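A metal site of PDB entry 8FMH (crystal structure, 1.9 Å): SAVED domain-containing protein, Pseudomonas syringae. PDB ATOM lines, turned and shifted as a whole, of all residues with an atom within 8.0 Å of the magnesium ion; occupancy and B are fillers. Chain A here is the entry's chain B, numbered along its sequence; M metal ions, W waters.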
ATOM      1  N   LEU A  58      -5.182  10.931  20.380  1.00  0.00           N
ATOM      2  CA  LEU A  58      -4.196  10.058  20.995  1.00  0.00           C
ATOM      3  C   LEU A  58      -2.847  10.766  21.165  1.00  0.00           C
ATOM      4  O   LEU A  58      -2.361  11.377  20.198  1.00  0.00           O
ATOM      5  CB  LEU A  58      -4.019   8.802  20.139  1.00  0.00           C
ATOM      6  CG  LEU A  58      -2.805   7.885  20.320  1.00  0.00           C
ATOM      7  CD1 LEU A  58      -2.625   7.443  21.759  1.00  0.00           C
ATOM      8  CD2 LEU A  58      -2.929   6.667  19.415  1.00  0.00           C
ATOM      9  N   PRO A  62       4.695   7.704  23.415  1.00  0.00           N
ATOM     10  CA  PRO A  62       4.331   6.808  24.519  1.00  0.00           C
ATOM     11  C   PRO A  62       4.427   7.475  25.888  1.00  0.00           C
ATOM     12  O   PRO A  62       4.992   8.569  25.992  1.00  0.00           O
ATOM     13  CB  PRO A  62       5.352   5.671  24.391  1.00  0.00           C
ATOM     14  CG  PRO A  62       5.817   5.714  22.981  1.00  0.00           C
ATOM     15  CD  PRO A  62       5.800   7.162  22.606  1.00  0.00           C
ATOM     16  N   HIS A  91      -5.813   4.262  14.235  1.00  0.00           N
ATOM     17  CA  HIS A  91      -5.712   4.041  15.670  1.00  0.00           C
ATOM     18  C   HIS A  91      -5.484   2.568  15.982  1.00  0.00           C
ATOM     19  O   HIS A  91      -4.696   2.228  16.876  1.00  0.00           O
ATOM     20  CB  HIS A  91      -6.972   4.540  16.373  1.00  0.00           C
ATOM     21  CG  HIS A  91      -6.920   4.423  17.868  1.00  0.00           C
ATOM     22  ND1 HIS A  91      -7.019   3.222  18.528  1.00  0.00           N
ATOM     23  CD2 HIS A  91      -6.795   5.369  18.826  1.00  0.00           C
ATOM     24  CE1 HIS A  91      -6.943   3.425  19.829  1.00  0.00           C
ATOM     25  NE2 HIS A  91      -6.805   4.721  20.042  1.00  0.00           N
ATOM     26  N   ILE A  94      -1.749   1.694  15.518  1.00  0.00           N
ATOM     27  CA  ILE A  94      -0.766   2.311  16.413  1.00  0.00           C
ATOM     28  C   ILE A  94      -0.940   1.752  17.817  1.00  0.00           C
ATOM     29  O   ILE A  94       0.006   1.218  18.397  1.00  0.00           O
ATOM     30  CB  ILE A  94      -0.902   3.840  16.411  1.00  0.00           C
ATOM     31  CG1 ILE A  94      -0.759   4.403  14.990  1.00  0.00           C
ATOM     32  CG2 ILE A  94       0.121   4.475  17.350  1.00  0.00           C
ATOM     33  CD1 ILE A  94       0.562   4.085  14.324  1.00  0.00           C
ATOM     34  N   ASP A  95      -2.143   1.891  18.373  1.00  0.00           N
ATOM     35  CA  ASP A  95      -2.416   1.476  19.748  1.00  0.00           C
ATOM     36  C   ASP A  95      -2.852   0.006  19.736  1.00  0.00           C
ATOM     37  O   ASP A  95      -4.039  -0.336  19.749  1.00  0.00           O
ATOM     38  CB  ASP A  95      -3.472   2.374  20.385  1.00  0.00           C
ATOM     39  CG  ASP A  95      -3.457   2.314  21.896  1.00  0.00           C
ATOM     40  OD1 ASP A  95      -2.497   1.760  22.473  1.00  0.00           O
ATOM     41  OD2 ASP A  95      -4.418   2.818  22.520  1.00  0.00           O
ATOM     42  N   ARG A  96      -1.854  -0.881  19.712  1.00  0.00           N
ATOM     43  CA  ARG A  96      -2.120  -2.316  19.643  1.00  0.00           C
ATOM     44  C   ARG A  96      -2.427  -2.910  21.014  1.00  0.00           C
ATOM     45  O   ARG A  96      -3.120  -3.935  21.096  1.00  0.00           O
ATOM     46  CB  ARG A  96      -0.950  -3.052  19.007  1.00  0.00           C
ATOM     47  CG  ARG A  96      -0.598  -2.593  17.604  1.00  0.00           C
ATOM     48  CD  ARG A  96       0.627  -1.681  17.599  1.00  0.00           C
ATOM     49  N   ASP A  97      -1.932  -2.297  22.089  1.00  0.00           N
ATOM     50  CA  ASP A  97      -2.253  -2.740  23.446  1.00  0.00           C
ATOM     51  C   ASP A  97      -3.382  -1.912  24.065  1.00  0.00           C
ATOM     52  O   ASP A  97      -3.613  -2.017  25.280  1.00  0.00           O
ATOM     53  CB  ASP A  97      -1.005  -2.682  24.336  1.00  0.00           C
ATOM     54  CG  ASP A  97      -0.491  -1.271  24.559  1.00  0.00           C
ATOM     55  OD1 ASP A  97      -0.653  -0.428  23.652  1.00  0.00           O
ATOM     56  OD2 ASP A  97       0.066  -1.008  25.642  1.00  0.00           O
ATOM     57  N   ALA A  98      -4.084  -1.112  23.261  1.00  0.00           N
ATOM     58  CA  ALA A  98      -5.216  -0.324  23.716  1.00  0.00           C
ATOM     59  C   ALA A  98      -4.976   0.305  25.089  1.00  0.00           C
ATOM     60  O   ALA A  98      -5.855   0.278  25.947  1.00  0.00           O
ATOM     61  CB  ALA A  98      -6.479  -1.185  23.757  1.00  0.00           C
ATOM     62  N   ASP A  99      -3.788   0.871  25.288  1.00  0.00           N
ATOM     63  CA  ASP A  99      -3.431   1.499  26.550  1.00  0.00           C
ATOM     64  C   ASP A  99      -3.535   3.017  26.492  1.00  0.00           C
ATOM     65  O   ASP A  99      -3.172   3.693  27.459  1.00  0.00           O
ATOM     66  CB  ASP A  99      -2.015   1.081  26.959  1.00  0.00           C
ATOM     67  CG  ASP A  99      -0.952   1.593  26.003  1.00  0.00           C
ATOM     68  OD1 ASP A  99      -1.273   1.854  24.831  1.00  0.00           O
ATOM     69  OD2 ASP A  99       0.221   1.719  26.436  1.00  0.00           O
ATOM     70  N   GLY A 100      -4.027   3.566  25.387  1.00  0.00           N
ATOM     71  CA  GLY A 100      -4.150   5.001  25.230  1.00  0.00           C
ATOM     72  C   GLY A 100      -2.901   5.709  24.768  1.00  0.00           C
ATOM     73  O   GLY A 100      -2.905   6.941  24.658  1.00  0.00           O
ATOM     74  N   TYR A 101      -1.833   4.976  24.484  1.00  0.00           N
ATOM     75  CA  TYR A 101      -0.570   5.551  24.043  1.00  0.00           C
ATOM     76  C   TYR A 101      -0.024   4.727  22.890  1.00  0.00           C
ATOM     77  O   TYR A 101      -0.381   3.557  22.719  1.00  0.00           O
ATOM     78  CB  TYR A 101       0.452   5.590  25.180  1.00  0.00           C
ATOM     79  CG  TYR A 101       0.217   6.699  26.185  1.00  0.00           C
ATOM     80  CD1 TYR A 101      -0.862   6.647  27.062  1.00  0.00           C
ATOM     81  CD2 TYR A 101       1.092   7.778  26.270  1.00  0.00           C
ATOM     82  CE1 TYR A 101      -1.070   7.657  27.985  1.00  0.00           C
ATOM     83  CE2 TYR A 101       0.879   8.791  27.185  1.00  0.00           C
ATOM     84  CZ  TYR A 101      -0.195   8.725  28.043  1.00  0.00           C
ATOM     85  OH  TYR A 101      -0.403   9.725  28.963  1.00  0.00           O
ATOM     86  N   PRO A 102       0.858   5.309  22.079  1.00  0.00           N
ATOM     87  CA  PRO A 102       1.445   4.581  20.958  1.00  0.00           C
ATOM     88  C   PRO A 102       2.618   3.719  21.403  1.00  0.00           C
ATOM     89  O   PRO A 102       3.152   3.859  22.506  1.00  0.00           O
ATOM     90  CB  PRO A 102       1.900   5.690  20.015  1.00  0.00           C
ATOM     91  CG  PRO A 102       2.251   6.816  20.932  1.00  0.00           C
ATOM     92  CD  PRO A 102       1.295   6.724  22.096  1.00  0.00           C
ATOM     93  N   GLU A 103       3.015   2.809  20.516  1.00  0.00           N
ATOM     94  CA  GLU A 103       4.178   1.964  20.759  1.00  0.00           C
ATOM     95  C   GLU A 103       5.479   2.609  20.332  1.00  0.00           C
ATOM     96  O   GLU A 103       6.550   2.211  20.805  1.00  0.00           O
ATOM     97  CB  GLU A 103       4.014   0.622  20.026  1.00  0.00           C
ATOM     98  CG  GLU A 103       2.597   0.069  20.014  1.00  0.00           C
ATOM     99  CD  GLU A 103       1.976   0.010  21.397  1.00  0.00           C
ATOM    100  OE1 GLU A 103       2.713  -0.285  22.368  1.00  0.00           O
ATOM    101  OE2 GLU A 103       0.750   0.270  21.531  1.00  0.00           O
ATOM    102  N   ASN A 104       5.409   3.615  19.452  1.00  0.00           N
ATOM    103  CA  ASN A 104       6.592   4.298  18.935  1.00  0.00           C
ATOM    104  C   ASN A 104       6.382   5.796  19.047  1.00  0.00           C
ATOM    105  O   ASN A 104       5.251   6.287  18.980  1.00  0.00           O
ATOM    106  CB  ASN A 104       6.857   3.927  17.477  1.00  0.00           C
ATOM    107  CG  ASN A 104       6.892   2.427  17.259  1.00  0.00           C
ATOM    108  OD1 ASN A 104       7.569   1.694  17.992  1.00  0.00           O
ATOM    109  ND2 ASN A 104       6.146   1.960  16.260  1.00  0.00           N
HETATM  110 MG    MG M   1      -0.420   1.517  22.899  1.00  0.00          MG
HETATM  111  O   HOH W   1       1.323   1.778  23.988  1.00  0.00           O
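The side-chain carboxylate (OD1) of Asp 95 lies close to the backbone NH (N) of Ala 98 (3.4 Å).
OD2 of Asp 95 lies within hydrogen-bond range of N of Gly 100 (3.0 Å).
The side-chain carboxylate (OE2) of Glu 103 sits close to the backbone NH (N) of Arg 96.
The magnesium ion is bound by the backbone carbonyl oxygen of Tyr 101 (2.0 Å), water W1 (2.1 Å), the side-chain carboxylate of Asp 97 (2.1 Å), the side-chain carboxylate of Asp 95 (2.1 Å), the side-chain carboxylate of Asp 99 (2.1 Å) and the side-chain carboxylate of Glu 103 (2.2 Å).
The magnesium ion has six donor atoms within binding distance.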
